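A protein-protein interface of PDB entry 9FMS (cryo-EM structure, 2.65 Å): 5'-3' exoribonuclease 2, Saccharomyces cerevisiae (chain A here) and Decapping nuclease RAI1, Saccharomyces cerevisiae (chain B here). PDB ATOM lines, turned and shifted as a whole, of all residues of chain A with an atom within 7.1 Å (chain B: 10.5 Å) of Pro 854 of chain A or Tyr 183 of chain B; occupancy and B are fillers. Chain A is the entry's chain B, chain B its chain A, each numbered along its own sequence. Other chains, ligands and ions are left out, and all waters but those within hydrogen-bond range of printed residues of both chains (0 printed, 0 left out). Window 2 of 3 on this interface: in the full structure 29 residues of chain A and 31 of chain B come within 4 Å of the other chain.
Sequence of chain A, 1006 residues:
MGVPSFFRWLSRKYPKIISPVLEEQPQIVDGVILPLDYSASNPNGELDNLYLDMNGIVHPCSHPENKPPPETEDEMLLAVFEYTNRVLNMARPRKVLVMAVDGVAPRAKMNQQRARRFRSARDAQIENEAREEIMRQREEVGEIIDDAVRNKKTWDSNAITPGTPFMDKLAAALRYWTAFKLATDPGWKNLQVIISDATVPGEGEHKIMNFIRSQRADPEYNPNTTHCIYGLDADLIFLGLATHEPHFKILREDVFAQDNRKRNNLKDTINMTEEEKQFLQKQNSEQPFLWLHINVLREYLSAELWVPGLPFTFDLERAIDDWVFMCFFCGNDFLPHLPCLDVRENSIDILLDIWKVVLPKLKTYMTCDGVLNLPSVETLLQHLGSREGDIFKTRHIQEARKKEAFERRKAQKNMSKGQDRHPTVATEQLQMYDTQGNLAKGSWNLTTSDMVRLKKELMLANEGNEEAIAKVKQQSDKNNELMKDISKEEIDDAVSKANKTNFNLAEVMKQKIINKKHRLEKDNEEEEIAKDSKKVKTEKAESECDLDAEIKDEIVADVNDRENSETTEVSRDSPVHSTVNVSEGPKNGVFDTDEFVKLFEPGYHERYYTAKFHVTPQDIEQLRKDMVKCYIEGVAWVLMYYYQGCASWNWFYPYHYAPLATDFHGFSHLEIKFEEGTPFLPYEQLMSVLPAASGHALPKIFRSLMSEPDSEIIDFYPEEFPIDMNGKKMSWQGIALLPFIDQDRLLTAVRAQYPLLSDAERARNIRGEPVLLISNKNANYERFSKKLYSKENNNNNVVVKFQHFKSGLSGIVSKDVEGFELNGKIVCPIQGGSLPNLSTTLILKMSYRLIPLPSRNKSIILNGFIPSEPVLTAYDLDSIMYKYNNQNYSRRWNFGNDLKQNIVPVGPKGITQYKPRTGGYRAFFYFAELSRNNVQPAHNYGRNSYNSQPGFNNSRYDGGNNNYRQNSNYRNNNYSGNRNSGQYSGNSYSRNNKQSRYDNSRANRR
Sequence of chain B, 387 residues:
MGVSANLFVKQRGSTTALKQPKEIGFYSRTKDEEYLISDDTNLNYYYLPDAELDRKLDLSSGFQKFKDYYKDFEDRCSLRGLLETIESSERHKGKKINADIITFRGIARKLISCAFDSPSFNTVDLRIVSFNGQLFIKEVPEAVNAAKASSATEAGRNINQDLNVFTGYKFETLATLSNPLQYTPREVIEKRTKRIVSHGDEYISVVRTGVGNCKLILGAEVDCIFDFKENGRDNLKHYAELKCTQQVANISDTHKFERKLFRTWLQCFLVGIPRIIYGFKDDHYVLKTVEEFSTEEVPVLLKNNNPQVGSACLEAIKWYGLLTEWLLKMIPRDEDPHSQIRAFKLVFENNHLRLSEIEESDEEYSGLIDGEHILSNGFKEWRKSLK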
ATOM      1  N   SER A 214      -1.400  24.082   9.363  1.00  0.00           N
ATOM      2  CA  SER A 214      -2.247  23.310  10.284  1.00  0.00           C
ATOM      3  C   SER A 214      -3.127  24.195  11.163  1.00  0.00           C
ATOM      4  O   SER A 214      -4.289  23.866  11.361  1.00  0.00           O
ATOM      5  CB  SER A 214      -1.413  22.371  11.148  1.00  0.00           C
ATOM      6  OG  SER A 214      -0.666  23.088  12.102  1.00  0.00           O
ATOM      7  N   ALA A 217      -6.213  25.445   9.221  1.00  0.00           N
ATOM      8  CA  ALA A 217      -7.196  24.408   8.923  1.00  0.00           C
ATOM      9  C   ALA A 217      -8.210  24.143  10.046  1.00  0.00           C
ATOM     10  O   ALA A 217      -9.153  23.386   9.843  1.00  0.00           O
ATOM     11  CB  ALA A 217      -6.440  23.137   8.563  1.00  0.00           C
ATOM     12  N   ASP A 218      -8.036  24.722  11.228  1.00  0.00           N
ATOM     13  CA  ASP A 218      -9.015  24.649  12.316  1.00  0.00           C
ATOM     14  C   ASP A 218     -10.220  25.562  12.014  1.00  0.00           C
ATOM     15  O   ASP A 218     -10.014  26.757  11.805  1.00  0.00           O
ATOM     16  CB  ASP A 218      -8.307  25.054  13.622  1.00  0.00           C
ATOM     17  CG  ASP A 218      -9.194  24.983  14.868  1.00  0.00           C
ATOM     18  OD1 ASP A 218     -10.401  24.692  14.731  1.00  0.00           O
ATOM     19  OD2 ASP A 218      -8.673  25.218  15.978  1.00  0.00           O
ATOM     20  N   PRO A 219     -11.476  25.079  12.008  1.00  0.00           N
ATOM     21  CA  PRO A 219     -12.648  25.937  11.858  1.00  0.00           C
ATOM     22  C   PRO A 219     -12.716  27.121  12.827  1.00  0.00           C
ATOM     23  O   PRO A 219     -13.270  28.157  12.478  1.00  0.00           O
ATOM     24  CB  PRO A 219     -13.849  25.023  12.071  1.00  0.00           C
ATOM     25  CG  PRO A 219     -13.340  23.663  11.630  1.00  0.00           C
ATOM     26  CD  PRO A 219     -11.885  23.686  12.078  1.00  0.00           C
ATOM     27  N   LYS A 801      -6.673  17.149  22.977  1.00  0.00           N
ATOM     28  CA  LYS A 801      -6.794  17.928  21.736  1.00  0.00           C
ATOM     29  C   LYS A 801      -7.441  19.273  22.041  1.00  0.00           C
ATOM     30  O   LYS A 801      -8.444  19.311  22.751  1.00  0.00           O
ATOM     31  CB  LYS A 801      -7.604  17.129  20.706  1.00  0.00           C
ATOM     32  CG  LYS A 801      -7.765  17.881  19.383  1.00  0.00           C
ATOM     33  CD  LYS A 801      -8.595  17.074  18.389  1.00  0.00           C
ATOM     34  CE  LYS A 801      -8.852  17.892  17.129  1.00  0.00           C
ATOM     35  NZ  LYS A 801      -9.774  17.214  16.201  1.00  0.00           N
ATOM     36  N   GLN A 803      -8.292  23.598  20.584  1.00  0.00           N
ATOM     37  CA  GLN A 803      -8.786  24.334  19.421  1.00  0.00           C
ATOM     38  C   GLN A 803      -8.558  25.841  19.569  1.00  0.00           C
ATOM     39  O   GLN A 803      -8.452  26.350  20.682  1.00  0.00           O
ATOM     40  CB  GLN A 803     -10.275  24.040  19.265  1.00  0.00           C
ATOM     41  CG  GLN A 803     -10.610  22.594  18.869  1.00  0.00           C
ATOM     42  CD  GLN A 803     -10.659  22.429  17.362  1.00  0.00           C
ATOM     43  OE1 GLN A 803      -9.862  21.728  16.757  1.00  0.00           O
ATOM     44  NE2 GLN A 803     -11.580  23.087  16.706  1.00  0.00           N
ATOM     45  N   ILE A 851      -2.403  19.017  14.765  1.00  0.00           N
ATOM     46  CA  ILE A 851      -3.598  18.338  14.259  1.00  0.00           C
ATOM     47  C   ILE A 851      -3.386  18.090  12.756  1.00  0.00           C
ATOM     48  O   ILE A 851      -3.124  19.049  12.026  1.00  0.00           O
ATOM     49  CB  ILE A 851      -4.874  19.157  14.539  1.00  0.00           C
ATOM     50  CG1 ILE A 851      -5.137  19.270  16.053  1.00  0.00           C
ATOM     51  CG2 ILE A 851      -6.099  18.509  13.878  1.00  0.00           C
ATOM     52  CD1 ILE A 851      -6.119  20.380  16.429  1.00  0.00           C
ATOM     53  N   PRO A 852      -3.472  16.844  12.260  1.00  0.00           N
ATOM     54  CA  PRO A 852      -3.231  16.551  10.853  1.00  0.00           C
ATOM     55  C   PRO A 852      -4.332  17.135   9.968  1.00  0.00           C
ATOM     56  O   PRO A 852      -5.490  17.206  10.377  1.00  0.00           O
ATOM     57  CB  PRO A 852      -3.150  15.027  10.768  1.00  0.00           C
ATOM     58  CG  PRO A 852      -4.007  14.557  11.939  1.00  0.00           C
ATOM     59  CD  PRO A 852      -3.771  15.630  12.993  1.00  0.00           C
ATOM     60  N   LEU A 853      -3.997  17.557   8.748  1.00  0.00           N
ATOM     61  CA  LEU A 853      -4.950  18.237   7.872  1.00  0.00           C
ATOM     62  C   LEU A 853      -6.138  17.331   7.492  1.00  0.00           C
ATOM     63  O   LEU A 853      -5.930  16.176   7.117  1.00  0.00           O
ATOM     64  CB  LEU A 853      -4.255  18.739   6.600  1.00  0.00           C
ATOM     65  CG  LEU A 853      -3.214  19.842   6.793  1.00  0.00           C
ATOM     66  CD1 LEU A 853      -2.602  20.190   5.443  1.00  0.00           C
ATOM     67  CD2 LEU A 853      -3.845  21.104   7.355  1.00  0.00           C
ATOM     68  N   PRO A 854      -7.380  17.839   7.520  1.00  0.00           N
ATOM     69  CA  PRO A 854      -8.569  17.077   7.145  1.00  0.00           C
ATOM     70  C   PRO A 854      -8.733  16.924   5.627  1.00  0.00           C
ATOM     71  O   PRO A 854      -9.468  16.057   5.161  1.00  0.00           O
ATOM     72  CB  PRO A 854      -9.726  17.877   7.739  1.00  0.00           C
ATOM     73  CG  PRO A 854      -9.232  19.318   7.661  1.00  0.00           C
ATOM     74  CD  PRO A 854      -7.746  19.178   7.950  1.00  0.00           C
ATOM     75  N   SER A 855      -8.080  17.787   4.853  1.00  0.00           N
ATOM     76  CA  SER A 855      -8.184  17.932   3.404  1.00  0.00           C
ATOM     77  C   SER A 855      -6.952  18.691   2.896  1.00  0.00           C
ATOM     78  O   SER A 855      -6.250  19.314   3.693  1.00  0.00           O
ATOM     79  CB  SER A 855      -9.467  18.709   3.083  1.00  0.00           C
ATOM     80  OG  SER A 855      -9.689  18.821   1.692  1.00  0.00           O
ATOM     81  N   ARG A 856      -6.661  18.690   1.594  1.00  0.00           N
ATOM     82  CA  ARG A 856      -5.594  19.536   1.037  1.00  0.00           C
ATOM     83  C   ARG A 856      -5.847  21.013   1.324  1.00  0.00           C
ATOM     84  O   ARG A 856      -6.963  21.503   1.183  1.00  0.00           O
ATOM     85  CB  ARG A 856      -5.448  19.306  -0.474  1.00  0.00           C
ATOM     86  CG  ARG A 856      -4.663  18.023  -0.739  1.00  0.00           C
ATOM     87  CD  ARG A 856      -4.429  17.798  -2.235  1.00  0.00           C
ATOM     88  NE  ARG A 856      -3.188  17.030  -2.430  1.00  0.00           N
ATOM     89  CZ  ARG A 856      -2.991  15.915  -3.102  1.00  0.00           C
ATOM     90  NH1 ARG A 856      -1.807  15.382  -3.115  1.00  0.00           N
ATOM     91  NH2 ARG A 856      -3.933  15.307  -3.764  1.00  0.00           N
ATOM     92  N   LYS A 858      -6.058  24.911   0.624  1.00  0.00           N
ATOM     93  CA  LYS A 858      -6.495  25.652  -0.563  1.00  0.00           C
ATOM     94  C   LYS A 858      -5.881  27.042  -0.614  1.00  0.00           C
ATOM     95  O   LYS A 858      -5.956  27.786   0.358  1.00  0.00           O
ATOM     96  CB  LYS A 858      -8.023  25.754  -0.573  1.00  0.00           C
ATOM     97  CG  LYS A 858      -8.709  24.407  -0.803  1.00  0.00           C
ATOM     98  CD  LYS A 858     -10.233  24.538  -0.839  1.00  0.00           C
ATOM     99  CE  LYS A 858     -10.851  24.910   0.513  1.00  0.00           C
ATOM    100  NZ  LYS A 858     -10.842  23.774   1.462  1.00  0.00           N
ATOM    101  N   TYR B  45     -22.955  26.692   5.662  1.00  0.00           N
ATOM    102  CA  TYR B  45     -21.861  27.504   6.180  1.00  0.00           C
ATOM    103  C   TYR B  45     -21.616  28.672   5.233  1.00  0.00           C
ATOM    104  O   TYR B  45     -21.639  28.486   4.021  1.00  0.00           O
ATOM    105  CB  TYR B  45     -20.612  26.630   6.338  1.00  0.00           C
ATOM    106  CG  TYR B  45     -20.787  25.494   7.325  1.00  0.00           C
ATOM    107  CD1 TYR B  45     -21.520  24.352   6.963  1.00  0.00           C
ATOM    108  CD2 TYR B  45     -20.258  25.593   8.619  1.00  0.00           C
ATOM    109  CE1 TYR B  45     -21.785  23.347   7.906  1.00  0.00           C
ATOM    110  CE2 TYR B  45     -20.507  24.584   9.566  1.00  0.00           C
ATOM    111  CZ  TYR B  45     -21.286  23.467   9.213  1.00  0.00           C
ATOM    112  OH  TYR B  45     -21.530  22.483  10.111  1.00  0.00           O
ATOM    113  N   TYR B  47     -19.803  31.423   2.906  1.00  0.00           N
ATOM    114  CA  TYR B  47     -18.540  31.732   2.242  1.00  0.00           C
ATOM    115  C   TYR B  47     -18.761  32.525   0.970  1.00  0.00           C
ATOM    116  O   TYR B  47     -19.268  31.981  -0.001  1.00  0.00           O
ATOM    117  CB  TYR B  47     -17.794  30.448   1.892  1.00  0.00           C
ATOM    118  CG  TYR B  47     -16.474  30.698   1.207  1.00  0.00           C
ATOM    119  CD1 TYR B  47     -15.461  31.346   1.918  1.00  0.00           C
ATOM    120  CD2 TYR B  47     -16.251  30.308  -0.121  1.00  0.00           C
ATOM    121  CE1 TYR B  47     -14.234  31.630   1.306  1.00  0.00           C
ATOM    122  CE2 TYR B  47     -15.024  30.586  -0.740  1.00  0.00           C
ATOM    123  CZ  TYR B  47     -14.018  31.256  -0.025  1.00  0.00           C
ATOM    124  OH  TYR B  47     -12.840  31.568  -0.605  1.00  0.00           O
ATOM    125  N   LEU B 177     -21.995  27.087   1.604  1.00  0.00           N
ATOM    126  CA  LEU B 177     -21.482  25.740   1.363  1.00  0.00           C
ATOM    127  C   LEU B 177     -22.254  24.750   2.240  1.00  0.00           C
ATOM    128  O   LEU B 177     -22.712  25.121   3.313  1.00  0.00           O
ATOM    129  CB  LEU B 177     -19.983  25.701   1.712  1.00  0.00           C
ATOM    130  CG  LEU B 177     -19.086  26.681   0.946  1.00  0.00           C
ATOM    131  CD1 LEU B 177     -17.682  26.678   1.537  1.00  0.00           C
ATOM    132  CD2 LEU B 177     -18.968  26.315  -0.526  1.00  0.00           C
ATOM    133  N   SER B 178     -22.396  23.491   1.837  1.00  0.00           N
ATOM    134  CA  SER B 178     -23.100  22.469   2.628  1.00  0.00           C
ATOM    135  C   SER B 178     -22.268  21.857   3.763  1.00  0.00           C
ATOM    136  O   SER B 178     -22.789  21.084   4.558  1.00  0.00           O
ATOM    137  CB  SER B 178     -23.578  21.358   1.698  1.00  0.00           C
ATOM    138  OG  SER B 178     -22.485  20.766   1.019  1.00  0.00           O
ATOM    139  N   ASN B 179     -20.974  22.158   3.835  1.00  0.00           N
ATOM    140  CA  ASN B 179     -19.997  21.667   4.810  1.00  0.00           C
ATOM    141  C   ASN B 179     -19.013  22.803   5.123  1.00  0.00           C
ATOM    142  O   ASN B 179     -18.923  23.736   4.326  1.00  0.00           O
ATOM    143  CB  ASN B 179     -19.254  20.447   4.242  1.00  0.00           C
ATOM    144  CG  ASN B 179     -20.157  19.284   3.887  1.00  0.00           C
ATOM    145  OD1 ASN B 179     -20.774  19.241   2.835  1.00  0.00           O
ATOM    146  ND2 ASN B 179     -20.249  18.290   4.731  1.00  0.00           N
ATOM    147  N   PRO B 180     -18.262  22.782   6.235  1.00  0.00           N
ATOM    148  CA  PRO B 180     -17.296  23.831   6.540  1.00  0.00           C
ATOM    149  C   PRO B 180     -16.311  24.068   5.395  1.00  0.00           C
ATOM    150  O   PRO B 180     -15.926  23.132   4.692  1.00  0.00           O
ATOM    151  CB  PRO B 180     -16.572  23.376   7.803  1.00  0.00           C
ATOM    152  CG  PRO B 180     -17.583  22.464   8.472  1.00  0.00           C
ATOM    153  CD  PRO B 180     -18.295  21.806   7.298  1.00  0.00           C
ATOM    154  N   LEU B 181     -15.839  25.298   5.216  1.00  0.00           N
ATOM    155  CA  LEU B 181     -14.872  25.623   4.169  1.00  0.00           C
ATOM    156  C   LEU B 181     -13.618  24.749   4.259  1.00  0.00           C
ATOM    157  O   LEU B 181     -13.102  24.259   3.257  1.00  0.00           O
ATOM    158  CB  LEU B 181     -14.527  27.111   4.293  1.00  0.00           C
ATOM    159  CG  LEU B 181     -13.483  27.600   3.280  1.00  0.00           C
ATOM    160  CD1 LEU B 181     -14.049  27.570   1.869  1.00  0.00           C
ATOM    161  CD2 LEU B 181     -13.091  29.028   3.620  1.00  0.00           C
ATOM    162  N   GLN B 182     -13.162  24.480   5.477  1.00  0.00           N
ATOM    163  CA  GLN B 182     -11.988  23.668   5.761  1.00  0.00           C
ATOM    164  C   GLN B 182     -12.138  22.207   5.313  1.00  0.00           C
ATOM    165  O   GLN B 182     -11.135  21.555   5.054  1.00  0.00           O
ATOM    166  CB  GLN B 182     -11.677  23.741   7.262  1.00  0.00           C
ATOM    167  CG  GLN B 182     -11.264  25.143   7.739  1.00  0.00           C
ATOM    168  CD  GLN B 182     -12.403  26.122   7.981  1.00  0.00           C
ATOM    169  OE1 GLN B 182     -13.581  25.797   7.955  1.00  0.00           O
ATOM    170  NE2 GLN B 182     -12.101  27.370   8.220  1.00  0.00           N
ATOM    171  N   TYR B 183     -13.363  21.692   5.186  1.00  0.00           N
ATOM    172  CA  TYR B 183     -13.661  20.306   4.800  1.00  0.00           C
ATOM    173  C   TYR B 183     -14.233  20.190   3.374  1.00  0.00           C
ATOM    174  O   TYR B 183     -14.692  19.121   2.977  1.00  0.00           O
ATOM    175  CB  TYR B 183     -14.599  19.658   5.831  1.00  0.00           C
ATOM    176  CG  TYR B 183     -14.227  19.766   7.299  1.00  0.00           C
ATOM    177  CD1 TYR B 183     -12.913  20.042   7.722  1.00  0.00           C
ATOM    178  CD2 TYR B 183     -15.233  19.588   8.264  1.00  0.00           C
ATOM    179  CE1 TYR B 183     -12.626  20.219   9.088  1.00  0.00           C
ATOM    180  CE2 TYR B 183     -14.945  19.733   9.633  1.00  0.00           C
ATOM    181  CZ  TYR B 183     -13.640  20.064  10.044  1.00  0.00           C
ATOM    182  OH  TYR B 183     -13.342  20.218  11.357  1.00  0.00           O
ATOM    183  N   THR B 184     -14.228  21.275   2.597  1.00  0.00           N
ATOM    184  CA  THR B 184     -14.807  21.333   1.247  1.00  0.00           C
ATOM    185  C   THR B 184     -13.708  21.334   0.181  1.00  0.00           C
ATOM    186  O   THR B 184     -12.843  22.211   0.239  1.00  0.00           O
ATOM    187  CB  THR B 184     -15.666  22.595   1.103  1.00  0.00           C
ATOM    188  OG1 THR B 184     -16.747  22.531   1.993  1.00  0.00           O
ATOM    189  CG2 THR B 184     -16.275  22.741  -0.282  1.00  0.00           C
ATOM    190  N   PRO B 185     -13.699  20.412  -0.796  1.00  0.00           N
ATOM    191  CA  PRO B 185     -12.692  20.388  -1.851  1.00  0.00           C
ATOM    192  C   PRO B 185     -12.910  21.497  -2.879  1.00  0.00           C
ATOM    193  O   PRO B 185     -14.037  21.917  -3.119  1.00  0.00           O
ATOM    194  CB  PRO B 185     -12.796  18.997  -2.469  1.00  0.00           C
ATOM    195  CG  PRO B 185     -14.255  18.632  -2.264  1.00  0.00           C
ATOM    196  CD  PRO B 185     -14.595  19.280  -0.931  1.00  0.00           C
ATOM    197  N   ARG B 186     -11.845  21.974  -3.527  1.00  0.00           N
ATOM    198  CA  ARG B 186     -11.886  23.178  -4.376  1.00  0.00           C
ATOM    199  C   ARG B 186     -12.846  23.079  -5.557  1.00  0.00           C
ATOM    200  O   ARG B 186     -13.466  24.069  -5.922  1.00  0.00           O
ATOM    201  CB  ARG B 186     -10.463  23.497  -4.847  1.00  0.00           C
ATOM    202  CG  ARG B 186     -10.391  24.894  -5.462  1.00  0.00           C
ATOM    203  CD  ARG B 186      -8.950  25.366  -5.640  1.00  0.00           C
ATOM    204  NE  ARG B 186      -8.947  26.779  -6.033  1.00  0.00           N
ATOM    205  CZ  ARG B 186      -8.233  27.747  -5.506  1.00  0.00           C
ATOM    206  NH1 ARG B 186      -8.511  28.984  -5.779  1.00  0.00           N
ATOM    207  NH2 ARG B 186      -7.237  27.546  -4.699  1.00  0.00           N
ATOM    208  N   GLU B 187     -13.042  21.891  -6.112  1.00  0.00           N
ATOM    209  CA  GLU B 187     -14.030  21.661  -7.174  1.00  0.00           C
ATOM    210  C   GLU B 187     -15.476  21.963  -6.743  1.00  0.00           C
ATOM    211  O   GLU B 187     -16.265  22.453  -7.544  1.00  0.00           O
ATOM    212  CB  GLU B 187     -13.902  20.221  -7.690  1.00  0.00           C
ATOM    213  CG  GLU B 187     -12.583  19.920  -8.434  1.00  0.00           C
ATOM    214  CD  GLU B 187     -12.454  18.470  -8.924  1.00  0.00           C
ATOM    215  OE1 GLU B 187     -13.347  17.656  -8.605  1.00  0.00           O
ATOM    216  OE2 GLU B 187     -11.490  18.143  -9.652  1.00  0.00           O
ATOM    217  N   VAL B 188     -15.847  21.744  -5.481  1.00  0.00           N
ATOM    218  CA  VAL B 188     -17.196  22.038  -4.975  1.00  0.00           C
ATOM    219  C   VAL B 188     -17.431  23.540  -4.884  1.00  0.00           C
ATOM    220  O   VAL B 188     -18.546  23.994  -5.116  1.00  0.00           O
ATOM    221  CB  VAL B 188     -17.429  21.334  -3.633  1.00  0.00           C
ATOM    222  CG1 VAL B 188     -18.724  21.748  -2.941  1.00  0.00           C
ATOM    223  CG2 VAL B 188     -17.513  19.824  -3.843  1.00  0.00           C
ATOM    224  N   ILE B 189     -16.388  24.330  -4.622  1.00  0.00           N
ATOM    225  CA  ILE B 189     -16.459  25.795  -4.639  1.00  0.00           C
ATOM    226  C   ILE B 189     -16.579  26.312  -6.077  1.00  0.00           C
ATOM    227  O   ILE B 189     -17.349  27.230  -6.337  1.00  0.00           O
ATOM    228  CB  ILE B 189     -15.257  26.410  -3.896  1.00  0.00           C
ATOM    229  CG1 ILE B 189     -15.225  25.924  -2.434  1.00  0.00           C
ATOM    230  CG2 ILE B 189     -15.322  27.942  -3.941  1.00  0.00           C
ATOM    231  CD1 ILE B 189     -14.012  26.391  -1.634  1.00  0.00           C
ATOM    232  N   ASP B 227     -19.345  31.857  11.266  1.00  0.00           N
ATOM    233  CA  ASP B 227     -17.950  31.625  11.636  1.00  0.00           C
ATOM    234  C   ASP B 227     -17.673  30.149  11.925  1.00  0.00           C
ATOM    235  O   ASP B 227     -16.986  29.510  11.135  1.00  0.00           O
ATOM    236  CB  ASP B 227     -17.479  32.609  12.716  1.00  0.00           C
ATOM    237  CG  ASP B 227     -17.344  34.065  12.288  1.00  0.00           C
ATOM    238  OD1 ASP B 227     -17.071  34.315  11.094  1.00  0.00           O
ATOM    239  OD2 ASP B 227     -17.518  34.960  13.140  1.00  0.00           O
ATOM    240  N   PHE B 228     -18.213  29.563  12.992  1.00  0.00           N
ATOM    241  CA  PHE B 228     -18.013  28.141  13.294  1.00  0.00           C
ATOM    242  C   PHE B 228     -19.134  27.521  14.123  1.00  0.00           C
ATOM    243  O   PHE B 228     -19.938  28.209  14.736  1.00  0.00           O
ATOM    244  CB  PHE B 228     -16.647  27.916  13.955  1.00  0.00           C
ATOM    245  CG  PHE B 228     -16.408  28.597  15.283  1.00  0.00           C
ATOM    246  CD1 PHE B 228     -15.853  29.882  15.317  1.00  0.00           C
ATOM    247  CD2 PHE B 228     -16.673  27.924  16.484  1.00  0.00           C
ATOM    248  CE1 PHE B 228     -15.577  30.502  16.542  1.00  0.00           C
ATOM    249  CE2 PHE B 228     -16.389  28.538  17.709  1.00  0.00           C
ATOM    250  CZ  PHE B 228     -15.840  29.825  17.740  1.00  0.00           C
ATOM    251  N   LYS B 229     -19.174  26.191  14.131  1.00  0.00           N
ATOM    252  CA  LYS B 229     -20.102  25.324  14.861  1.00  0.00           C
ATOM    253  C   LYS B 229     -19.448  24.840  16.151  1.00  0.00           C
ATOM    254  O   LYS B 229     -18.295  24.422  16.137  1.00  0.00           O
ATOM    255  CB  LYS B 229     -20.435  24.145  13.930  1.00  0.00           C
ATOM    256  CG  LYS B 229     -21.230  22.982  14.526  1.00  0.00           C
ATOM    257  CD  LYS B 229     -22.742  23.142  14.447  1.00  0.00           C
ATOM    258  CE  LYS B 229     -23.350  21.980  15.226  1.00  0.00           C
ATOM    259  NZ  LYS B 229     -24.771  21.760  14.909  1.00  0.00           N
ATOM    260  N   GLU B 230     -20.189  24.824  17.248  1.00  0.00           N
ATOM    261  CA  GLU B 230     -19.825  24.131  18.484  1.00  0.00           C
ATOM    262  C   GLU B 230     -20.750  22.931  18.695  1.00  0.00           C
ATOM    263  O   GLU B 230     -21.968  23.090  18.741  1.00  0.00           O
ATOM    264  CB  GLU B 230     -19.931  25.093  19.671  1.00  0.00           C
ATOM    265  CG  GLU B 230     -18.989  26.286  19.546  1.00  0.00           C
ATOM    266  CD  GLU B 230     -19.093  27.201  20.767  1.00  0.00           C
ATOM    267  OE1 GLU B 230     -18.710  26.773  21.875  1.00  0.00           O
ATOM    268  OE2 GLU B 230     -19.542  28.360  20.610  1.00  0.00           O
ATOM    269  N   ASN B 231     -20.222  21.716  18.812  1.00  0.00           N
ATOM    270  CA  ASN B 231     -21.051  20.519  18.981  1.00  0.00           C
ATOM    271  C   ASN B 231     -21.671  20.448  20.382  1.00  0.00           C
ATOM    272  O   ASN B 231     -20.992  20.681  21.377  1.00  0.00           O
ATOM    273  CB  ASN B 231     -20.235  19.257  18.677  1.00  0.00           C
ATOM    274  CG  ASN B 231     -19.781  19.203  17.235  1.00  0.00           C
ATOM    275  OD1 ASN B 231     -18.771  19.777  16.861  1.00  0.00           O
ATOM    276  ND2 ASN B 231     -20.513  18.536  16.377  1.00  0.00           N
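O of Asn 179 of chain B is in hydrogen-bond range of OG1 of Thr 184 of chain B (3.4 Å).
O of Pro 180 of chain B sits at hydrogen-bond distance from OG1 of Thr 184 of chain B (2.9 Å).
Printed residues of chain B within 4 Å of Pro 854 of chain A: Gln 182 and Tyr 183.
Of chain B, only Gln 182 (3.8 Å) comes within 4 Å of Ser 855 of chain A.
Printed residues of chain B within 4 Å of Pro 219 of chain A: Gln 182 (3.9 Å), Tyr 183 (3.5 Å) and Phe 228 (3.7 Å).
Of the printed residues of chain A, Gln 182 of chain B touches Ala 217, Pro 219, Pro 854 and Ser 855.
Arg 856 of chain A touches none of the printed residues of chain B.
Tyr 45 of chain B touches none of the printed residues of chain A.
The nearest residue of chain B that does not touch Pro 854 of chain A is Thr 184 of chain B (7.4 Å).
The nearest residue of chain A that does not touch Tyr 183 of chain B is Ala 217 of chain A (4.8 Å).
Of the 20 printed residues of chain B, 5 touch a printed residue of chain A.
Printed residues of chain B that touch a printed residue of chain A: Leu 181, Gln 182, Tyr 183, Thr 184 and Phe 228.
Printed residues of chain A that touch a printed residue of chain B: Ala 217, Pro 219, Pro 854, Ser 855 and Lys 858.
Hydrophobic or aromatic side chains of chain A that line the printed part of chain B: Pro 219 and Pro 854.
Along chain A the printed residues that touch a printed residue of chain B span positions 217 to 858.
Among the printed residues, 9 pairs touch across the chains.
Among the printed residues, no Asp or Glu carboxylate lies within 4 Å of a Lys or Arg side-chain nitrogen of the other chain.
CG of Gln 182 of chain B touches O of Ala 217 of chain A, 3.5 Å away.
Pro 219 of chain A touches Gln 182 of chain B.
OH of Tyr 183 of chain B touches CG of Pro 219 of chain A (3.5 Å).
Pro 219 of chain A touches Phe 228 of chain B.
Gln 182 of chain B touches Pro 854 of chain A (O to CG, 3.9 Å).
CD1 of Tyr 183 of chain B touches CG of Pro 854 of chain A (3.8 Å).
Ser 855 of chain A touches Gln 182 of chain B.
O of Leu 181 of chain B sits at hydrogen-bond distance from NZ of Lys 858 of chain A.
NZ of Lys 858 of chain A lies within hydrogen-bond range of O of Thr 184 of chain B.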
